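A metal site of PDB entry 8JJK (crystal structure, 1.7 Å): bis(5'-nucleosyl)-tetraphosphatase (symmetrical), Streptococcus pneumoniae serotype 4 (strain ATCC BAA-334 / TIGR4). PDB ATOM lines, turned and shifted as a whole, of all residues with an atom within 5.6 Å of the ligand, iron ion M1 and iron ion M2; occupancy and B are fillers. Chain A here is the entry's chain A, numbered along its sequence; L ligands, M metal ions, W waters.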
ATOM      1  N   ARG A  26     -25.796 -14.764 -18.569  1.00  0.00           N
ATOM      2  CA  ARG A  26     -25.669 -15.620 -17.400  1.00  0.00           C
ATOM      3  C   ARG A  26     -25.716 -17.111 -17.780  1.00  0.00           C
ATOM      4  O   ARG A  26     -24.953 -17.907 -17.239  1.00  0.00           O
ATOM      5  CB  ARG A  26     -26.722 -15.265 -16.342  1.00  0.00           C
ATOM      6  CG  ARG A  26     -26.602 -16.035 -15.026  1.00  0.00           C
ATOM      7  CD  ARG A  26     -25.241 -15.877 -14.365  1.00  0.00           C
ATOM      8  NE  ARG A  26     -24.917 -14.469 -14.145  1.00  0.00           N
ATOM      9  CZ  ARG A  26     -23.760 -14.029 -13.644  1.00  0.00           C
ATOM     10  NH1 ARG A  26     -22.807 -14.883 -13.284  1.00  0.00           N
ATOM     11  NH2 ARG A  26     -23.558 -12.728 -13.488  1.00  0.00           N
ATOM     12  N   HIS A  29     -22.488 -18.051 -19.342  1.00  0.00           N
ATOM     13  CA  HIS A  29     -21.537 -18.233 -18.239  1.00  0.00           C
ATOM     14  C   HIS A  29     -21.677 -19.620 -17.626  1.00  0.00           C
ATOM     15  O   HIS A  29     -20.676 -20.309 -17.396  1.00  0.00           O
ATOM     16  CB  HIS A  29     -21.734 -17.140 -17.185  1.00  0.00           C
ATOM     17  CG  HIS A  29     -21.098 -17.428 -15.858  1.00  0.00           C
ATOM     18  ND1 HIS A  29     -19.727 -17.465 -15.682  1.00  0.00           N
ATOM     19  CD2 HIS A  29     -21.635 -17.672 -14.636  1.00  0.00           C
ATOM     20  CE1 HIS A  29     -19.456 -17.711 -14.411  1.00  0.00           C
ATOM     21  NE2 HIS A  29     -20.596 -17.830 -13.760  1.00  0.00           N
ATOM     22  N   VAL A  33     -18.967 -22.574 -17.285  1.00  0.00           N
ATOM     23  CA  VAL A  33     -18.556 -23.228 -16.027  1.00  0.00           C
ATOM     24  C   VAL A  33     -18.733 -24.749 -16.129  1.00  0.00           C
ATOM     25  O   VAL A  33     -17.917 -25.501 -15.621  1.00  0.00           O
ATOM     26  CB  VAL A  33     -19.289 -22.623 -14.799  1.00  0.00           C
ATOM     27  CG1 VAL A  33     -18.875 -23.299 -13.501  1.00  0.00           C
ATOM     28  CG2 VAL A  33     -19.011 -21.129 -14.723  1.00  0.00           C
ATOM     29  N   HIS A  58     -24.599 -23.860 -10.952  1.00  0.00           N
ATOM     30  CA  HIS A  58     -24.087 -23.115  -9.801  1.00  0.00           C
ATOM     31  C   HIS A  58     -24.794 -21.750  -9.620  1.00  0.00           C
ATOM     32  O   HIS A  58     -25.028 -21.323  -8.494  1.00  0.00           O
ATOM     33  CB  HIS A  58     -22.556 -22.968  -9.864  1.00  0.00           C
ATOM     34  CG  HIS A  58     -22.110 -21.884 -10.780  1.00  0.00           C
ATOM     35  ND1 HIS A  58     -22.209 -21.975 -12.148  1.00  0.00           N
ATOM     36  CD2 HIS A  58     -21.611 -20.656 -10.522  1.00  0.00           C
ATOM     37  CE1 HIS A  58     -21.778 -20.849 -12.696  1.00  0.00           C
ATOM     38  NE2 HIS A  58     -21.398 -20.037 -11.726  1.00  0.00           N
ATOM     39  N   ASP A  59     -25.141 -21.108 -10.739  1.00  0.00           N
ATOM     40  CA  ASP A  59     -25.775 -19.779 -10.740  1.00  0.00           C
ATOM     41  C   ASP A  59     -27.262 -19.839 -11.089  1.00  0.00           C
ATOM     42  O   ASP A  59     -27.853 -18.818 -11.484  1.00  0.00           O
ATOM     43  CB  ASP A  59     -25.043 -18.810 -11.683  1.00  0.00           C
ATOM     44  CG  ASP A  59     -23.867 -18.077 -11.016  1.00  0.00           C
ATOM     45  OD1 ASP A  59     -23.737 -18.090  -9.766  1.00  0.00           O
ATOM     46  OD2 ASP A  59     -23.073 -17.478 -11.768  1.00  0.00           O
ATOM     47  N   LYS A  62     -29.435 -17.170  -9.488  1.00  0.00           N
ATOM     48  CA  LYS A  62     -28.863 -15.824  -9.563  1.00  0.00           C
ATOM     49  C   LYS A  62     -29.913 -14.709  -9.606  1.00  0.00           C
ATOM     50  O   LYS A  62     -29.687 -13.628  -9.058  1.00  0.00           O
ATOM     51  CB  LYS A  62     -27.919 -15.704 -10.773  1.00  0.00           C
ATOM     52  CG  LYS A  62     -27.076 -14.431 -10.843  1.00  0.00           C
ATOM     53  CD  LYS A  62     -25.950 -14.385  -9.807  1.00  0.00           C
ATOM     54  CE  LYS A  62     -25.050 -13.177 -10.074  1.00  0.00           C
ATOM     55  NZ  LYS A  62     -23.832 -13.119  -9.216  1.00  0.00           N
ATOM     56  N   TRP A  85     -27.401  -9.822   4.626  1.00  0.00           N
ATOM     57  CA  TRP A  85     -26.604  -9.791   3.404  1.00  0.00           C
ATOM     58  C   TRP A  85     -27.500  -9.647   2.174  1.00  0.00           C
ATOM     59  O   TRP A  85     -28.558  -9.014   2.262  1.00  0.00           O
ATOM     60  CB  TRP A  85     -25.684 -11.016   3.376  1.00  0.00           C
ATOM     61  CG  TRP A  85     -24.817 -11.015   4.591  1.00  0.00           C
ATOM     62  CD1 TRP A  85     -25.131 -11.527   5.833  1.00  0.00           C
ATOM     63  CD2 TRP A  85     -23.543 -10.409   4.734  1.00  0.00           C
ATOM     64  NE1 TRP A  85     -24.116 -11.288   6.718  1.00  0.00           N
ATOM     65  CE2 TRP A  85     -23.127 -10.608   6.071  1.00  0.00           C
ATOM     66  CE3 TRP A  85     -22.688  -9.732   3.844  1.00  0.00           C
ATOM     67  CZ2 TRP A  85     -21.886 -10.156   6.548  1.00  0.00           C
ATOM     68  CZ3 TRP A  85     -21.455  -9.283   4.315  1.00  0.00           C
ATOM     69  CH2 TRP A  85     -21.073  -9.481   5.658  1.00  0.00           C
ATOM     70  N   ASN A  88     -25.353 -11.715  -3.522  1.00  0.00           N
ATOM     71  CA  ASN A  88     -23.999 -12.294  -3.612  1.00  0.00           C
ATOM     72  C   ASN A  88     -23.846 -13.515  -2.726  1.00  0.00           C
ATOM     73  O   ASN A  88     -23.392 -14.568  -3.185  1.00  0.00           O
ATOM     74  CB  ASN A  88     -22.910 -11.272  -3.247  1.00  0.00           C
ATOM     75  CG  ASN A  88     -22.741 -10.185  -4.273  1.00  0.00           C
ATOM     76  OD1 ASN A  88     -23.297 -10.240  -5.379  1.00  0.00           O
ATOM     77  ND2 ASN A  88     -21.950  -9.178  -3.921  1.00  0.00           N
ATOM     78  N   VAL A  89     -24.233 -13.374  -1.453  1.00  0.00           N
ATOM     79  CA  VAL A  89     -24.206 -14.473  -0.507  1.00  0.00           C
ATOM     80  C   VAL A  89     -25.349 -15.453  -0.795  1.00  0.00           C
ATOM     81  O   VAL A  89     -25.128 -16.674  -0.808  1.00  0.00           O
ATOM     82  CB  VAL A  89     -24.252 -13.979   0.963  1.00  0.00           C
ATOM     83  CG1 VAL A  89     -24.326 -15.139   1.943  1.00  0.00           C
ATOM     84  CG2 VAL A  89     -23.038 -13.099   1.294  1.00  0.00           C
ATOM     85  N   HIS A  91     -27.356 -16.360  -3.428  1.00  0.00           N
ATOM     86  CA  HIS A  91     -27.714 -17.139  -4.631  1.00  0.00           C
ATOM     87  C   HIS A  91     -27.131 -18.551  -4.582  1.00  0.00           C
ATOM     88  O   HIS A  91     -27.730 -19.488  -5.095  1.00  0.00           O
ATOM     89  CB  HIS A  91     -27.442 -16.381  -5.936  1.00  0.00           C
ATOM     90  CG  HIS A  91     -25.990 -16.304  -6.308  1.00  0.00           C
ATOM     91  ND1 HIS A  91     -25.130 -15.404  -5.731  1.00  0.00           N
ATOM     92  CD2 HIS A  91     -25.271 -16.982  -7.231  1.00  0.00           C
ATOM     93  CE1 HIS A  91     -23.924 -15.547  -6.262  1.00  0.00           C
ATOM     94  NE2 HIS A  91     -23.988 -16.492  -7.173  1.00  0.00           N
ATOM     95  N   HIS A 117     -20.026 -21.902  -3.660  1.00  0.00           N
ATOM     96  CA  HIS A 117     -19.272 -21.523  -4.877  1.00  0.00           C
ATOM     97  C   HIS A 117     -18.817 -20.064  -4.880  1.00  0.00           C
ATOM     98  O   HIS A 117     -17.865 -19.710  -5.579  1.00  0.00           O
ATOM     99  CB  HIS A 117     -20.048 -21.838  -6.153  1.00  0.00           C
ATOM    100  CG  HIS A 117     -21.040 -20.786  -6.525  1.00  0.00           C
ATOM    101  ND1 HIS A 117     -22.369 -20.860  -6.185  1.00  0.00           N
ATOM    102  CD2 HIS A 117     -20.901 -19.612  -7.201  1.00  0.00           C
ATOM    103  CE1 HIS A 117     -23.011 -19.795  -6.635  1.00  0.00           C
ATOM    104  NE2 HIS A 117     -22.133 -19.022  -7.260  1.00  0.00           N
ATOM    105  N   THR A 118     -19.492 -19.219  -4.101  1.00  0.00           N
ATOM    106  CA  THR A 118     -19.135 -17.803  -4.003  1.00  0.00           C
ATOM    107  C   THR A 118     -18.127 -17.541  -2.878  1.00  0.00           C
ATOM    108  O   THR A 118     -17.110 -16.873  -3.088  1.00  0.00           O
ATOM    109  CB  THR A 118     -20.389 -16.938  -3.757  1.00  0.00           C
ATOM    110  OG1 THR A 118     -21.381 -17.230  -4.743  1.00  0.00           O
ATOM    111  CG2 THR A 118     -20.053 -15.443  -3.766  1.00  0.00           C
ATOM    112  N   VAL A 119     -18.426 -18.060  -1.699  1.00  0.00           N
ATOM    113  CA  VAL A 119     -17.680 -17.710  -0.484  1.00  0.00           C
ATOM    114  C   VAL A 119     -16.655 -18.749  -0.044  1.00  0.00           C
ATOM    115  O   VAL A 119     -15.805 -18.471   0.809  1.00  0.00           O
ATOM    116  CB  VAL A 119     -18.649 -17.411   0.695  1.00  0.00           C
ATOM    117  CG1 VAL A 119     -19.540 -16.209   0.362  1.00  0.00           C
ATOM    118  CG2 VAL A 119     -19.498 -18.632   1.038  1.00  0.00           C
ATOM    119  N   ASP A 135     -15.763 -21.399 -11.922  1.00  0.00           N
ATOM    120  CA  ASP A 135     -16.582 -20.197 -11.970  1.00  0.00           C
ATOM    121  C   ASP A 135     -15.730 -18.978 -12.379  1.00  0.00           C
ATOM    122  O   ASP A 135     -16.177 -18.090 -13.139  1.00  0.00           O
ATOM    123  CB  ASP A 135     -17.195 -19.978 -10.579  1.00  0.00           C
ATOM    124  CG  ASP A 135     -18.176 -18.836 -10.522  1.00  0.00           C
ATOM    125  OD1 ASP A 135     -18.818 -18.493 -11.547  1.00  0.00           O
ATOM    126  OD2 ASP A 135     -18.325 -18.306  -9.398  1.00  0.00           O
ATOM    127  N   ARG A 141     -15.017 -15.399 -19.200  1.00  0.00           N
ATOM    128  CA  ARG A 141     -14.474 -14.388 -18.269  1.00  0.00           C
ATOM    129  C   ARG A 141     -13.288 -13.671 -18.908  1.00  0.00           C
ATOM    130  O   ARG A 141     -12.482 -14.301 -19.600  1.00  0.00           O
ATOM    131  CB  ARG A 141     -14.071 -15.031 -16.942  1.00  0.00           C
ATOM    132  CG  ARG A 141     -15.225 -15.558 -16.089  1.00  0.00           C
ATOM    133  CD  ARG A 141     -15.748 -14.501 -15.118  1.00  0.00           C
ATOM    134  NE  ARG A 141     -16.244 -15.142 -13.909  1.00  0.00           N
ATOM    135  CZ  ARG A 141     -17.447 -14.964 -13.366  1.00  0.00           C
ATOM    136  NH1 ARG A 141     -18.325 -14.097 -13.901  1.00  0.00           N
ATOM    137  NH2 ARG A 141     -17.767 -15.632 -12.272  1.00  0.00           N
ATOM    138  N   GLU A 164      -7.719 -17.023  -6.275  1.00  0.00           N
ATOM    139  CA  GLU A 164      -9.058 -16.444  -6.445  1.00  0.00           C
ATOM    140  C   GLU A 164      -9.532 -15.748  -5.175  1.00  0.00           C
ATOM    141  O   GLU A 164     -10.082 -14.631  -5.227  1.00  0.00           O
ATOM    142  CB  GLU A 164     -10.069 -17.505  -6.883  1.00  0.00           C
ATOM    143  CG  GLU A 164     -11.485 -16.950  -6.967  1.00  0.00           C
ATOM    144  CD  GLU A 164     -12.549 -17.967  -7.380  1.00  0.00           C
ATOM    145  OE1 GLU A 164     -12.191 -19.097  -7.788  1.00  0.00           O
ATOM    146  OE2 GLU A 164     -13.739 -17.623  -7.296  1.00  0.00           O
ATOM    147  N   THR A 168     -10.307 -11.773  -4.567  1.00  0.00           N
ATOM    148  CA  THR A 168     -11.653 -11.367  -4.199  1.00  0.00           C
ATOM    149  C   THR A 168     -11.671 -10.513  -2.942  1.00  0.00           C
ATOM    150  O   THR A 168     -12.343  -9.458  -2.920  1.00  0.00           O
ATOM    151  CB  THR A 168     -12.554 -12.587  -4.101  1.00  0.00           C
ATOM    152  OG1 THR A 168     -12.624 -13.164  -5.413  1.00  0.00           O
ATOM    153  CG2 THR A 168     -13.960 -12.202  -3.622  1.00  0.00           C
ATOM    154  N   LEU A 172     -12.844  -6.650  -3.021  1.00  0.00           N
ATOM    155  CA  LEU A 172     -13.956  -6.175  -2.173  1.00  0.00           C
ATOM    156  C   LEU A 172     -13.510  -5.014  -1.293  1.00  0.00           C
ATOM    157  O   LEU A 172     -14.211  -4.004  -1.184  1.00  0.00           O
ATOM    158  CB  LEU A 172     -14.564  -7.328  -1.372  1.00  0.00           C
ATOM    159  CG  LEU A 172     -15.312  -8.375  -2.208  1.00  0.00           C
ATOM    160  CD1 LEU A 172     -15.676  -9.530  -1.291  1.00  0.00           C
ATOM    161  CD2 LEU A 172     -16.550  -7.824  -2.900  1.00  0.00           C
ATOM    162  N   PRO A 178     -18.850  -4.775   1.938  1.00  0.00           N
ATOM    163  CA  PRO A 178     -18.794  -5.723   3.056  1.00  0.00           C
ATOM    164  C   PRO A 178     -18.316  -7.085   2.580  1.00  0.00           C
ATOM    165  O   PRO A 178     -18.606  -7.483   1.430  1.00  0.00           O
ATOM    166  CB  PRO A 178     -20.251  -5.817   3.522  1.00  0.00           C
ATOM    167  CG  PRO A 178     -20.926  -4.596   3.008  1.00  0.00           C
ATOM    168  CD  PRO A 178     -20.187  -4.172   1.773  1.00  0.00           C
ATOM    169  N   ILE A 179     -17.571  -7.790   3.438  1.00  0.00           N
ATOM    170  CA  ILE A 179     -17.009  -9.098   3.128  1.00  0.00           C
ATOM    171  C   ILE A 179     -17.660 -10.142   4.043  1.00  0.00           C
ATOM    172  O   ILE A 179     -17.490 -10.106   5.255  1.00  0.00           O
ATOM    173  CB  ILE A 179     -15.467  -9.115   3.271  1.00  0.00           C
ATOM    174  CG1 ILE A 179     -14.861  -8.133   2.261  1.00  0.00           C
ATOM    175  CG2 ILE A 179     -14.903 -10.533   3.089  1.00  0.00           C
ATOM    176  CD1 ILE A 179     -13.423  -7.741   2.534  1.00  0.00           C
ATOM    177  N   TYR A 180     -18.403 -11.069   3.437  1.00  0.00           N
ATOM    178  CA  TYR A 180     -19.045 -12.138   4.207  1.00  0.00           C
ATOM    179  C   TYR A 180     -17.974 -12.930   4.947  1.00  0.00           C
ATOM    180  O   TYR A 180     -16.958 -13.297   4.354  1.00  0.00           O
ATOM    181  CB  TYR A 180     -19.889 -13.026   3.285  1.00  0.00           C
ATOM    182  CG  TYR A 180     -20.750 -13.998   4.043  1.00  0.00           C
ATOM    183  CD1 TYR A 180     -21.839 -13.549   4.780  1.00  0.00           C
ATOM    184  CD2 TYR A 180     -20.476 -15.365   4.018  1.00  0.00           C
ATOM    185  CE1 TYR A 180     -22.642 -14.435   5.495  1.00  0.00           C
ATOM    186  CE2 TYR A 180     -21.288 -16.265   4.718  1.00  0.00           C
ATOM    187  CZ  TYR A 180     -22.367 -15.795   5.449  1.00  0.00           C
ATOM    188  OH  TYR A 180     -23.145 -16.683   6.137  1.00  0.00           O
ATOM    189  N   PRO A 181     -18.134 -13.123   6.266  1.00  0.00           N
ATOM    190  CA  PRO A 181     -17.032 -13.687   7.042  1.00  0.00           C
ATOM    191  C   PRO A 181     -16.550 -15.064   6.585  1.00  0.00           C
ATOM    192  O   PRO A 181     -15.366 -15.360   6.743  1.00  0.00           O
ATOM    193  CB  PRO A 181     -17.584 -13.708   8.470  1.00  0.00           C
ATOM    194  CG  PRO A 181     -18.449 -12.492   8.485  1.00  0.00           C
ATOM    195  CD  PRO A 181     -19.165 -12.559   7.155  1.00  0.00           C
ATOM    196  N   THR A 183     -15.904 -16.019   3.689  1.00  0.00           N
ATOM    197  CA  THR A 183     -14.819 -15.776   2.740  1.00  0.00           C
ATOM    198  C   THR A 183     -13.460 -15.650   3.418  1.00  0.00           C
ATOM    199  O   THR A 183     -12.457 -16.129   2.891  1.00  0.00           O
ATOM    200  CB  THR A 183     -15.129 -14.560   1.864  1.00  0.00           C
ATOM    201  OG1 THR A 183     -16.187 -14.913   0.984  1.00  0.00           O
ATOM    202  CG2 THR A 183     -13.934 -14.119   1.018  1.00  0.00           C
HETATM  203  P1  LIG L   1     -20.973 -14.939 -10.271  1.00  0.00           P
HETATM  204  O1  LIG L   1     -20.956 -13.456 -10.559  1.00  0.00           O
HETATM  205  O2  LIG L   1     -22.254 -15.445  -9.600  1.00  0.00           O
HETATM  206  O3  LIG L   1     -20.597 -15.716 -11.518  1.00  0.00           O
HETATM  207  P2  LIG L   1     -19.695 -15.402  -7.658  1.00  0.00           P
HETATM  208  O4  LIG L   1     -18.352 -15.967  -7.275  1.00  0.00           O
HETATM  209  O5  LIG L   1     -20.934 -16.138  -7.237  1.00  0.00           O
HETATM  210  O6  LIG L   1     -19.709 -15.105  -9.253  1.00  0.00           O
HETATM  211  O7  LIG L   1     -19.715 -13.917  -7.068  1.00  0.00           O
HETATM  212  C1  LIG L   1     -20.864 -13.075  -7.096  1.00  0.00           C
HETATM  213  C2  LIG L   1     -20.425 -11.742  -6.495  1.00  0.00           C
HETATM  214  O8  LIG L   1     -20.238 -11.944  -5.097  1.00  0.00           O
HETATM  215  C3  LIG L   1     -19.100 -11.181  -7.049  1.00  0.00           C
HETATM  216  O9  LIG L   1     -19.294  -9.801  -7.397  1.00  0.00           O
HETATM  217  C4  LIG L   1     -18.109 -11.327  -5.898  1.00  0.00           C
HETATM  218  O10 LIG L   1     -17.111 -10.298  -5.798  1.00  0.00           O
HETATM  219  C5  LIG L   1     -19.036 -11.278  -4.687  1.00  0.00           C
HETATM  220  N1  LIG L   1     -18.450 -11.839  -3.451  1.00  0.00           N
HETATM  221  C6  LIG L   1     -17.554 -12.839  -3.344  1.00  0.00           C
HETATM  222  N2  LIG L   1     -17.249 -13.083  -2.050  1.00  0.00           N
HETATM  223  C7  LIG L   1     -17.954 -12.202  -1.332  1.00  0.00           C
HETATM  224  C8  LIG L   1     -18.108 -11.861   0.092  1.00  0.00           C
HETATM  225  N3  LIG L   1     -17.434 -12.541   1.006  1.00  0.00           N
HETATM  226  N4  LIG L   1     -18.947 -10.862   0.448  1.00  0.00           N
HETATM  227  C9  LIG L   1     -19.629 -10.171  -0.477  1.00  0.00           C
HETATM  228  N5  LIG L   1     -19.562 -10.403  -1.800  1.00  0.00           N
HETATM  229  C10 LIG L   1     -18.744 -11.387  -2.251  1.00  0.00           C
HETATM  230 FE    FE M   1     -20.867 -17.897 -11.645  1.00  0.00          FE
HETATM  231 FE    FE M   2     -22.353 -17.207  -8.447  1.00  0.00          FE
HETATM  232 MG    MG M   3     -16.406 -18.326  -7.288  1.00  0.00          MG
HETATM  233  O   HOH W   1     -20.591  -7.173  -0.270  1.00  0.00           O
HETATM  234  O   HOH W   2     -20.853 -17.750  -9.687  1.00  0.00           O
HETATM  235  O   HOH W   3     -16.087 -16.151  -9.591  1.00  0.00           O
HETATM  236  O   HOH W   4     -19.464  -7.263  -5.308  1.00  0.00           O
HETATM  237  O   HOH W   5     -16.661 -14.598  -6.038  1.00  0.00           O
HETATM  238  O   HOH W   6     -20.449 -11.846 -12.603  1.00  0.00           O
HETATM  239  O   HOH W   7     -18.457 -12.421 -10.231  1.00  0.00           O
HETATM  240  O   HOH W   8     -15.625 -14.983  -1.747  1.00  0.00           O
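OG1 of Thr 118 touches iron ion M2, 3.8 Å away. Along chain A the residues within 4 Å of iron ion M2 span positions 59 to 118. The nearest printed residue that does not touch iron ion M2 is His 58 (4.1 Å).
Thr 168 touches the ligand. CD1 of Leu 172 touches C7 of the ligand (3.5 Å). Pro 178 touches the ligand (O to C9, 3.5 Å). CA of Ile 179 touches N4 of the ligand (3.7 Å). Hydrophobic or aromatic side chains that line the ligand: His 29, His 91, His 117, Leu 172, Ile 179 and Tyr 180. 16 residues have an atom within 4 Å of the ligand: Arg 26, His 29, Asp 59, Lys 62, Asn 88, His 91, His 117, Thr 118, Asp 135, Arg 141, Thr 168, Leu 172, Pro 178, Ile 179, Tyr 180 and Thr 183.
Water W2 bridges OD2 of Asp 135 and O6 of the ligand. Water W8 lies within hydrogen-bond range of a nitrogen (N2) of the ligand (2.5 Å), the backbone carbonyl oxygen of Thr 118 (2.8 Å) and the side-chain hydroxyl of Thr 183 (2.8 Å). Water W6 lies within hydrogen-bond range of O1 of the ligand (2.7 Å), NH2 of Arg 26 (3.4 Å) and NH1 of Arg 141 (3.4 Å). Water W3 lies within hydrogen-bond range of OD2 of Asp 135, NH2 of Arg 141 and O4 of the ligand. Water W4 bridges O9 of the ligand (3.3 Å) and ND2 of Asn 88 (3.4 Å).
OG1 of Thr 118 sits close to O5 of the ligand, at 2.8 Å. An oxygen (O1) of the ligand is in salt-bridge range of the guanidinium group (NH1) of Arg 26. An oxygen (O3) of the ligand lies close to the guanidinium group (NH2) of Arg 141, at 2.9 Å. The side-chain hydroxyl (OG1) of Thr 183 lies within hydrogen-bond range of a nitrogen (N3) of the ligand (2.7 Å). The side-chain amino group (NZ) of Lys 62 lies within salt-bridge range of an oxygen (O1) of the ligand, at 3.2 Å. ND2 of Asn 88 sits at hydrogen-bond distance from N5 of the ligand. O of Tyr 180 lies close to N3 of the ligand (3.5 Å). N of Tyr 180 is in hydrogen-bond range of N4 of the ligand (3.0 Å).
NH1 of Arg 26 touches iron ion M1, 3.9 Å away. NH2 of Arg 141 touches iron ion M1 (3.9 Å). Of the 23 residues printed, 6 come within 4 Å of iron ion M1. The nearest printed residue that does not touch iron ion M1 is His 117 (4.7 Å).
Iron ion M2 is bound by water W2 (2.0 Å), the side-chain carboxylate of Asp 59 (2.1 Å), an oxygen (O2) of the ligand (2.1 Å), an oxygen (O5) of the ligand (2.1 Å), a ring nitrogen (NE2) of His 117 (2.2 Å) and a ring nitrogen (NE2) of His 91 (2.2 Å).
Iron ion M1 is bound by water W2 (2.0 Å), a ring nitrogen (NE2) of His 29 (2.1 Å), the side-chain carboxylate (OD1) of Asp 135 (2.1 Å), an oxygen (O3) of the ligand (2.2 Å), a ring nitrogen (NE2) of His 58 (2.2 Å) and the side-chain carboxylate (OD2) of Asp 59 (2.2 Å). Iron ion M1 has six donor atoms within binding distance.
The backbone carbonyl oxygen (O) of Glu 164 is in hydrogen-bond range of the side-chain hydroxyl (OG1) of Thr 168, at 2.9 Å. A ring nitrogen (ND1) of His 91 sits at hydrogen-bond distance from the backbone carbonyl oxygen (O) of Asn 88 (3.2 Å). OD2 of Asp 135 is in salt-bridge range of NH2 of Arg 141 (3.97 Å). OG1 of Thr 118 sits close to NE2 of His 117. The guanidinium group of Arg 26 sits close to the side-chain carboxylate of Asp 59, 3.0 Å away.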
